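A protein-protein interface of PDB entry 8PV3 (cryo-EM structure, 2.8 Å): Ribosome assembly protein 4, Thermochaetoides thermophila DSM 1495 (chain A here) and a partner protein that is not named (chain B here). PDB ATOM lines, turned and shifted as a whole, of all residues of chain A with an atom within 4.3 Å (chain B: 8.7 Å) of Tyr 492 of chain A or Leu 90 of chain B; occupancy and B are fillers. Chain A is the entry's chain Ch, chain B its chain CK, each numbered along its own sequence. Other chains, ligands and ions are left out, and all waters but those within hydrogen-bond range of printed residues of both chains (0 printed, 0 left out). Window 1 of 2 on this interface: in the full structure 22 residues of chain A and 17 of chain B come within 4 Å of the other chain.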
ATOM      1  N   PRO A 148      11.695 -20.183 -37.781  1.00  0.00           N
ATOM      2  CA  PRO A 148      11.911 -21.507 -37.179  1.00  0.00           C
ATOM      3  C   PRO A 148      10.934 -22.569 -37.661  1.00  0.00           C
ATOM      4  O   PRO A 148       9.753 -22.304 -37.889  1.00  0.00           O
ATOM      5  CB  PRO A 148      11.732 -21.238 -35.684  1.00  0.00           C
ATOM      6  CG  PRO A 148      12.200 -19.869 -35.515  1.00  0.00           C
ATOM      7  CD  PRO A 148      11.800 -19.127 -36.752  1.00  0.00           C
ATOM      8  N   ILE A 149      11.456 -23.785 -37.818  1.00  0.00           N
ATOM      9  CA  ILE A 149      10.658 -24.913 -38.280  1.00  0.00           C
ATOM     10  C   ILE A 149       9.837 -25.461 -37.123  1.00  0.00           C
ATOM     11  O   ILE A 149      10.366 -25.723 -36.036  1.00  0.00           O
ATOM     12  CB  ILE A 149      11.567 -25.995 -38.872  1.00  0.00           C
ATOM     13  CG1 ILE A 149      12.415 -25.409 -39.993  1.00  0.00           C
ATOM     14  CG2 ILE A 149      10.751 -27.167 -39.379  1.00  0.00           C
ATOM     15  CD1 ILE A 149      13.497 -26.324 -40.441  1.00  0.00           C
ATOM     16  N   TRP A 424      10.443 -32.547 -19.332  1.00  0.00           N
ATOM     17  CA  TRP A 424      11.114 -31.273 -19.122  1.00  0.00           C
ATOM     18  C   TRP A 424      12.164 -31.345 -18.022  1.00  0.00           C
ATOM     19  O   TRP A 424      12.831 -30.343 -17.749  1.00  0.00           O
ATOM     20  CB  TRP A 424      10.089 -30.183 -18.793  1.00  0.00           C
ATOM     21  CG  TRP A 424       9.265 -29.731 -19.966  1.00  0.00           C
ATOM     22  CD1 TRP A 424       8.529 -30.514 -20.804  1.00  0.00           C
ATOM     23  CD2 TRP A 424       9.074 -28.384 -20.407  1.00  0.00           C
ATOM     24  NE1 TRP A 424       7.902 -29.741 -21.747  1.00  0.00           N
ATOM     25  CE2 TRP A 424       8.221 -28.428 -21.525  1.00  0.00           C
ATOM     26  CE3 TRP A 424       9.548 -27.145 -19.970  1.00  0.00           C
ATOM     27  CZ2 TRP A 424       7.831 -27.283 -22.211  1.00  0.00           C
ATOM     28  CZ3 TRP A 424       9.160 -26.010 -20.652  1.00  0.00           C
ATOM     29  CH2 TRP A 424       8.310 -26.087 -21.760  1.00  0.00           C
ATOM     30  N   TYR A 450      12.301 -32.178 -26.086  1.00  0.00           N
ATOM     31  CA  TYR A 450      11.051 -31.797 -26.724  1.00  0.00           C
ATOM     32  C   TYR A 450      10.403 -32.932 -27.495  1.00  0.00           C
ATOM     33  O   TYR A 450       9.189 -33.130 -27.368  1.00  0.00           O
ATOM     34  CB  TYR A 450      11.275 -30.607 -27.656  1.00  0.00           C
ATOM     35  CG  TYR A 450      11.351 -29.288 -26.929  1.00  0.00           C
ATOM     36  CD1 TYR A 450      10.570 -29.050 -25.808  1.00  0.00           C
ATOM     37  CD2 TYR A 450      12.192 -28.277 -27.370  1.00  0.00           C
ATOM     38  CE1 TYR A 450      10.633 -27.848 -25.139  1.00  0.00           C
ATOM     39  CE2 TYR A 450      12.258 -27.068 -26.708  1.00  0.00           C
ATOM     40  CZ  TYR A 450      11.476 -26.861 -25.594  1.00  0.00           C
ATOM     41  OH  TYR A 450      11.537 -25.659 -24.930  1.00  0.00           O
ATOM     42  N   GLN A 451      11.156 -33.688 -28.291  1.00  0.00           N
ATOM     43  CA  GLN A 451      10.509 -34.749 -29.053  1.00  0.00           C
ATOM     44  C   GLN A 451      11.327 -36.027 -29.001  1.00  0.00           C
ATOM     45  O   GLN A 451      12.534 -36.012 -28.758  1.00  0.00           O
ATOM     46  CB  GLN A 451      10.262 -34.340 -30.509  1.00  0.00           C
ATOM     47  CG  GLN A 451       9.027 -33.485 -30.694  1.00  0.00           C
ATOM     48  CD  GLN A 451       8.490 -33.536 -32.103  1.00  0.00           C
ATOM     49  OE1 GLN A 451       9.033 -34.230 -32.961  1.00  0.00           O
ATOM     50  NE2 GLN A 451       7.410 -32.807 -32.351  1.00  0.00           N
ATOM     51  N   GLU A 490      17.525 -24.223 -30.667  1.00  0.00           N
ATOM     52  CA  GLU A 490      16.677 -25.274 -30.112  1.00  0.00           C
ATOM     53  C   GLU A 490      16.078 -26.148 -31.207  1.00  0.00           C
ATOM     54  O   GLU A 490      15.812 -25.687 -32.320  1.00  0.00           O
ATOM     55  CB  GLU A 490      15.554 -24.661 -29.278  1.00  0.00           C
ATOM     56  CG  GLU A 490      16.012 -23.624 -28.273  1.00  0.00           C
ATOM     57  CD  GLU A 490      14.866 -23.066 -27.457  1.00  0.00           C
ATOM     58  OE1 GLU A 490      13.793 -23.699 -27.434  1.00  0.00           O
ATOM     59  OE2 GLU A 490      15.037 -21.994 -26.842  1.00  0.00           O
ATOM     60  N   VAL A 491      15.869 -27.420 -30.882  1.00  0.00           N
ATOM     61  CA  VAL A 491      15.314 -28.389 -31.820  1.00  0.00           C
ATOM     62  C   VAL A 491      13.835 -28.570 -31.516  1.00  0.00           C
ATOM     63  O   VAL A 491      13.461 -28.956 -30.404  1.00  0.00           O
ATOM     64  CB  VAL A 491      16.061 -29.729 -31.732  1.00  0.00           C
ATOM     65  CG1 VAL A 491      15.458 -30.731 -32.690  1.00  0.00           C
ATOM     66  CG2 VAL A 491      17.533 -29.533 -32.022  1.00  0.00           C
ATOM     67  N   TYR A 492      12.989 -28.297 -32.508  1.00  0.00           N
ATOM     68  CA  TYR A 492      11.547 -28.348 -32.327  1.00  0.00           C
ATOM     69  C   TYR A 492      10.903 -29.616 -32.857  1.00  0.00           C
ATOM     70  O   TYR A 492      10.038 -30.176 -32.183  1.00  0.00           O
ATOM     71  CB  TYR A 492      10.879 -27.147 -33.007  1.00  0.00           C
ATOM     72  CG  TYR A 492      11.040 -25.847 -32.260  1.00  0.00           C
ATOM     73  CD1 TYR A 492      11.134 -25.828 -30.876  1.00  0.00           C
ATOM     74  CD2 TYR A 492      11.077 -24.636 -32.937  1.00  0.00           C
ATOM     75  CE1 TYR A 492      11.276 -24.643 -30.189  1.00  0.00           C
ATOM     76  CE2 TYR A 492      11.217 -23.446 -32.257  1.00  0.00           C
ATOM     77  CZ  TYR A 492      11.315 -23.456 -30.884  1.00  0.00           C
ATOM     78  OH  TYR A 492      11.452 -22.271 -30.202  1.00  0.00           O
ATOM     79  N   ALA A 493      11.294 -30.082 -34.039  1.00  0.00           N
ATOM     80  CA  ALA A 493      10.646 -31.213 -34.683  1.00  0.00           C
ATOM     81  C   ALA A 493      11.674 -32.276 -35.030  1.00  0.00           C
ATOM     82  O   ALA A 493      12.717 -31.979 -35.621  1.00  0.00           O
ATOM     83  CB  ALA A 493       9.901 -30.773 -35.941  1.00  0.00           C
ATOM     84  N   GLY A 506      14.502 -30.262 -37.153  1.00  0.00           N
ATOM     85  CA  GLY A 506      14.382 -28.845 -37.436  1.00  0.00           C
ATOM     86  C   GLY A 506      14.051 -28.097 -36.170  1.00  0.00           C
ATOM     87  O   GLY A 506      13.563 -28.677 -35.196  1.00  0.00           O
ATOM     88  N   GLY A 507      14.310 -26.795 -36.185  1.00  0.00           N
ATOM     89  CA  GLY A 507      14.017 -25.990 -35.021  1.00  0.00           C
ATOM     90  C   GLY A 507      14.237 -24.506 -35.205  1.00  0.00           C
ATOM     91  O   GLY A 507      13.966 -23.950 -36.272  1.00  0.00           O
ATOM     92  N   LYS A 508      14.746 -23.857 -34.157  1.00  0.00           N
ATOM     93  CA  LYS A 508      14.863 -22.406 -34.121  1.00  0.00           C
ATOM     94  C   LYS A 508      15.948 -21.865 -35.043  1.00  0.00           C
ATOM     95  O   LYS A 508      15.978 -20.656 -35.296  1.00  0.00           O
ATOM     96  CB  LYS A 508      15.122 -21.961 -32.681  1.00  0.00           C
ATOM     97  CG  LYS A 508      14.560 -20.608 -32.310  1.00  0.00           C
ATOM     98  CD  LYS A 508      14.699 -20.370 -30.817  1.00  0.00           C
ATOM     99  CE  LYS A 508      14.344 -18.945 -30.442  1.00  0.00           C
ATOM    100  NZ  LYS A 508      14.613 -18.675 -29.005  1.00  0.00           N
ATOM    101  N   PRO B  82       1.683 -15.083 -30.160  1.00  0.00           N
ATOM    102  CA  PRO B  82       3.035 -14.756 -29.711  1.00  0.00           C
ATOM    103  C   PRO B  82       3.831 -13.994 -30.761  1.00  0.00           C
ATOM    104  O   PRO B  82       3.299 -13.668 -31.821  1.00  0.00           O
ATOM    105  CB  PRO B  82       3.650 -16.132 -29.454  1.00  0.00           C
ATOM    106  CG  PRO B  82       2.479 -17.006 -29.083  1.00  0.00           C
ATOM    107  CD  PRO B  82       1.207 -16.339 -29.560  1.00  0.00           C
ATOM    108  N   ASP B  84       7.670 -14.741 -31.381  1.00  0.00           N
ATOM    109  CA  ASP B  84       8.546 -15.744 -31.971  1.00  0.00           C
ATOM    110  C   ASP B  84       7.748 -16.999 -32.315  1.00  0.00           C
ATOM    111  O   ASP B  84       6.897 -17.423 -31.530  1.00  0.00           O
ATOM    112  CB  ASP B  84       9.680 -16.096 -31.013  1.00  0.00           C
ATOM    113  CG  ASP B  84      10.599 -17.166 -31.567  1.00  0.00           C
ATOM    114  OD1 ASP B  84      11.421 -16.843 -32.450  1.00  0.00           O
ATOM    115  OD2 ASP B  84      10.502 -18.328 -31.119  1.00  0.00           O
ATOM    116  N   PRO B  85       7.985 -17.594 -33.484  1.00  0.00           N
ATOM    117  CA  PRO B  85       7.269 -18.825 -33.846  1.00  0.00           C
ATOM    118  C   PRO B  85       7.662 -19.989 -32.947  1.00  0.00           C
ATOM    119  O   PRO B  85       8.838 -20.339 -32.829  1.00  0.00           O
ATOM    120  CB  PRO B  85       7.695 -19.062 -35.298  1.00  0.00           C
ATOM    121  CG  PRO B  85       8.076 -17.715 -35.799  1.00  0.00           C
ATOM    122  CD  PRO B  85       8.710 -17.025 -34.632  1.00  0.00           C
ATOM    123  N   ILE B  86       6.659 -20.586 -32.312  1.00  0.00           N
ATOM    124  CA  ILE B  86       6.859 -21.709 -31.399  1.00  0.00           C
ATOM    125  C   ILE B  86       5.882 -22.812 -31.786  1.00  0.00           C
ATOM    126  O   ILE B  86       4.815 -22.540 -32.356  1.00  0.00           O
ATOM    127  CB  ILE B  86       6.665 -21.286 -29.923  1.00  0.00           C
ATOM    128  CG1 ILE B  86       5.345 -20.537 -29.749  1.00  0.00           C
ATOM    129  CG2 ILE B  86       7.838 -20.450 -29.445  1.00  0.00           C
ATOM    130  CD1 ILE B  86       5.056 -20.136 -28.326  1.00  0.00           C
ATOM    131  N   PRO B  87       6.218 -24.070 -31.501  1.00  0.00           N
ATOM    132  CA  PRO B  87       5.303 -25.165 -31.841  1.00  0.00           C
ATOM    133  C   PRO B  87       4.068 -25.194 -30.951  1.00  0.00           C
ATOM    134  O   PRO B  87       3.911 -24.411 -30.009  1.00  0.00           O
ATOM    135  CB  PRO B  87       6.153 -26.424 -31.644  1.00  0.00           C
ATOM    136  CG  PRO B  87       7.548 -25.964 -31.588  1.00  0.00           C
ATOM    137  CD  PRO B  87       7.531 -24.575 -31.066  1.00  0.00           C
ATOM    138  N   SER B  88       3.177 -26.133 -31.284  1.00  0.00           N
ATOM    139  CA  SER B  88       1.891 -26.238 -30.603  1.00  0.00           C
ATOM    140  C   SER B  88       2.048 -26.630 -29.141  1.00  0.00           C
ATOM    141  O   SER B  88       1.261 -26.190 -28.296  1.00  0.00           O
ATOM    142  CB  SER B  88       0.998 -27.246 -31.324  1.00  0.00           C
ATOM    143  OG  SER B  88       0.668 -26.795 -32.623  1.00  0.00           O
ATOM    144  N   TYR B  89       3.045 -27.454 -28.820  1.00  0.00           N
ATOM    145  CA  TYR B  89       3.257 -27.819 -27.427  1.00  0.00           C
ATOM    146  C   TYR B  89       3.882 -26.695 -26.616  1.00  0.00           C
ATOM    147  O   TYR B  89       3.845 -26.751 -25.384  1.00  0.00           O
ATOM    148  CB  TYR B  89       4.112 -29.086 -27.328  1.00  0.00           C
ATOM    149  CG  TYR B  89       5.440 -29.047 -28.057  1.00  0.00           C
ATOM    150  CD1 TYR B  89       6.569 -28.494 -27.466  1.00  0.00           C
ATOM    151  CD2 TYR B  89       5.571 -29.594 -29.324  1.00  0.00           C
ATOM    152  CE1 TYR B  89       7.782 -28.471 -28.125  1.00  0.00           C
ATOM    153  CE2 TYR B  89       6.779 -29.576 -29.987  1.00  0.00           C
ATOM    154  CZ  TYR B  89       7.879 -29.012 -29.383  1.00  0.00           C
ATOM    155  OH  TYR B  89       9.083 -28.994 -30.045  1.00  0.00           O
ATOM    156  N   LEU B  90       4.451 -25.684 -27.268  1.00  0.00           N
ATOM    157  CA  LEU B  90       4.975 -24.509 -26.589  1.00  0.00           C
ATOM    158  C   LEU B  90       4.005 -23.339 -26.608  1.00  0.00           C
ATOM    159  O   LEU B  90       4.231 -22.356 -25.898  1.00  0.00           O
ATOM    160  CB  LEU B  90       6.305 -24.081 -27.212  1.00  0.00           C
ATOM    161  CG  LEU B  90       7.513 -24.974 -26.940  1.00  0.00           C
ATOM    162  CD1 LEU B  90       8.768 -24.345 -27.509  1.00  0.00           C
ATOM    163  CD2 LEU B  90       7.664 -25.231 -25.456  1.00  0.00           C
ATOM    164  N   LEU B  91       2.943 -23.416 -27.406  1.00  0.00           N
ATOM    165  CA  LEU B  91       1.926 -22.372 -27.402  1.00  0.00           C
ATOM    166  C   LEU B  91       1.178 -22.345 -26.074  1.00  0.00           C
ATOM    167  O   LEU B  91       1.054 -23.360 -25.383  1.00  0.00           O
ATOM    168  CB  LEU B  91       0.936 -22.581 -28.546  1.00  0.00           C
ATOM    169  CG  LEU B  91       1.402 -22.174 -29.942  1.00  0.00           C
ATOM    170  CD1 LEU B  91       0.413 -22.652 -30.981  1.00  0.00           C
ATOM    171  CD2 LEU B  91       1.574 -20.674 -30.028  1.00  0.00           C
ATOM    172  N   ASP B  92       0.699 -21.150 -25.717  1.00  0.00           N
ATOM    173  CA  ASP B  92      -0.077 -20.807 -24.523  1.00  0.00           C
ATOM    174  C   ASP B  92       0.703 -20.951 -23.221  1.00  0.00           C
ATOM    175  O   ASP B  92       0.106 -20.816 -22.149  1.00  0.00           O
ATOM    176  CB  ASP B  92      -1.378 -21.616 -24.404  1.00  0.00           C
ATOM    177  CG  ASP B  92      -2.423 -21.186 -25.409  1.00  0.00           C
ATOM    178  OD1 ASP B  92      -2.583 -19.964 -25.613  1.00  0.00           O
ATOM    179  OD2 ASP B  92      -3.084 -22.068 -25.995  1.00  0.00           O
ATOM    180  N   ARG B  93       2.003 -21.209 -23.269  1.00  0.00           N
ATOM    181  CA  ARG B  93       2.832 -21.256 -22.076  1.00  0.00           C
ATOM    182  C   ARG B  93       3.523 -19.915 -21.863  1.00  0.00           C
ATOM    183  O   ARG B  93       3.593 -19.074 -22.762  1.00  0.00           O
ATOM    184  CB  ARG B  93       3.879 -22.368 -22.176  1.00  0.00           C
ATOM    185  CG  ARG B  93       3.319 -23.753 -22.430  1.00  0.00           C
ATOM    186  CD  ARG B  93       4.436 -24.783 -22.445  1.00  0.00           C
ATOM    187  NE  ARG B  93       3.942 -26.140 -22.645  1.00  0.00           N
ATOM    188  CZ  ARG B  93       3.545 -26.946 -21.671  1.00  0.00           C
ATOM    189  NH1 ARG B  93       3.586 -26.572 -20.404  1.00  0.00           N
ATOM    190  NH2 ARG B  93       3.101 -28.162 -21.976  1.00  0.00           N
ATOM    191  N   ALA B  94       4.037 -19.725 -20.652  1.00  0.00           N
ATOM    192  CA  ALA B  94       4.782 -18.515 -20.326  1.00  0.00           C
ATOM    193  C   ALA B  94       6.211 -18.652 -20.832  1.00  0.00           C
ATOM    194  O   ALA B  94       6.998 -19.435 -20.291  1.00  0.00           O
ATOM    195  CB  ALA B  94       4.755 -18.267 -18.821  1.00  0.00           C
ATOM    196  N   ASN B  95       6.551 -17.894 -21.871  1.00  0.00           N
ATOM    197  CA  ASN B  95       7.859 -17.950 -22.493  1.00  0.00           C
ATOM    198  C   ASN B  95       8.541 -16.593 -22.386  1.00  0.00           C
ATOM    199  O   ASN B  95       7.851 -15.566 -22.313  1.00  0.00           O
ATOM    200  CB  ASN B  95       7.742 -18.366 -23.972  1.00  0.00           C
ATOM    201  CG  ASN B  95       7.043 -19.699 -24.148  1.00  0.00           C
ATOM    202  OD1 ASN B  95       6.132 -19.833 -24.964  1.00  0.00           O
ATOM    203  ND2 ASN B  95       7.473 -20.696 -23.387  1.00  0.00           N
ATOM    204  N   THR B  98      12.549 -12.690 -25.211  1.00  0.00           N
ATOM    205  CA  THR B  98      13.719 -12.852 -26.084  1.00  0.00           C
ATOM    206  C   THR B  98      13.944 -11.594 -26.930  1.00  0.00           C
ATOM    207  O   THR B  98      13.787 -11.606 -28.155  1.00  0.00           O
ATOM    208  CB  THR B  98      13.603 -14.114 -26.951  1.00  0.00           C
ATOM    209  OG1 THR B  98      13.255 -15.223 -26.115  1.00  0.00           O
ATOM    210  CG2 THR B  98      14.949 -14.460 -27.598  1.00  0.00           C
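The backbone carbonyl oxygen (O) of Tyr 89 of chain B is in hydrogen-bond range of the guanidinium group (NE) of Arg 93 of chain B (2.8 Å). The side-chain amide oxygen (OD1) of Asn 95 of chain B sits close to the backbone carbonyl oxygen (O) of Leu 90 of chain B (3.3 Å). OE2 of Glu 490 of chain A lies within salt-bridge range of NZ of Lys 508 of chain A, 3.98 Å away. The backbone carbonyl oxygen (O) of Gly 506 of chain A sits at hydrogen-bond distance from the backbone NH (N) of Tyr 492 of chain A, at 2.8 Å.
Tyr 492 of chain A touches just these residues of chain B: Pro 85 (3.95 Å), Pro 87 (3.6 Å), Tyr 89 (2.6 Å) and Leu 90 (3.7 Å). No residue of chain B comes within 4 Å of Gly 507 of chain A. Of the printed residues of chain A, Pro 85 of chain B touches Tyr 492. Printed residues of chain A within 4 Å of Pro 87 of chain B: Tyr 492 (3.6 Å). The nearest residue of chain B that does not touch Tyr 492 of chain A is Ile 86 of chain B (4.1 Å). The nearest printed residue of chain A that does not touch Leu 90 of chain B is Glu 490 of chain A (5.1 Å). The nearest printed residue of chain A that does not touch Tyr 89 of chain B is Gln 451 of chain A (4.1 Å).
Among the printed residues, pairs that only touch across the chains: Trp 424 of chain A with Leu 90 of chain B (3.8 Å), Tyr 450 of chain A with Tyr 89 of chain B (3.6 Å), Tyr 450 of chain A with Leu 90 of chain B (3.9 Å), Tyr 492 of chain A with Pro 85 of chain B (3.95 Å), Tyr 492 of chain A with Pro 87 of chain B (3.6 Å), Tyr 492 of chain A with Leu 90 of chain B (3.7 Å) and Lys 508 of chain A with Asp 84 of chain B (3.9 Å).
Among the printed residues, 8 pairs touch across the chains. Among the printed residues, no Asp or Glu carboxylate lies within 4 Å of a Lys or Arg side-chain nitrogen of the other chain.
The side-chain hydroxyl (OH) of Tyr 89 of chain B lies within hydrogen-bond range of the backbone carbonyl oxygen (O) of Tyr 492 of chain A (2.6 Å).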
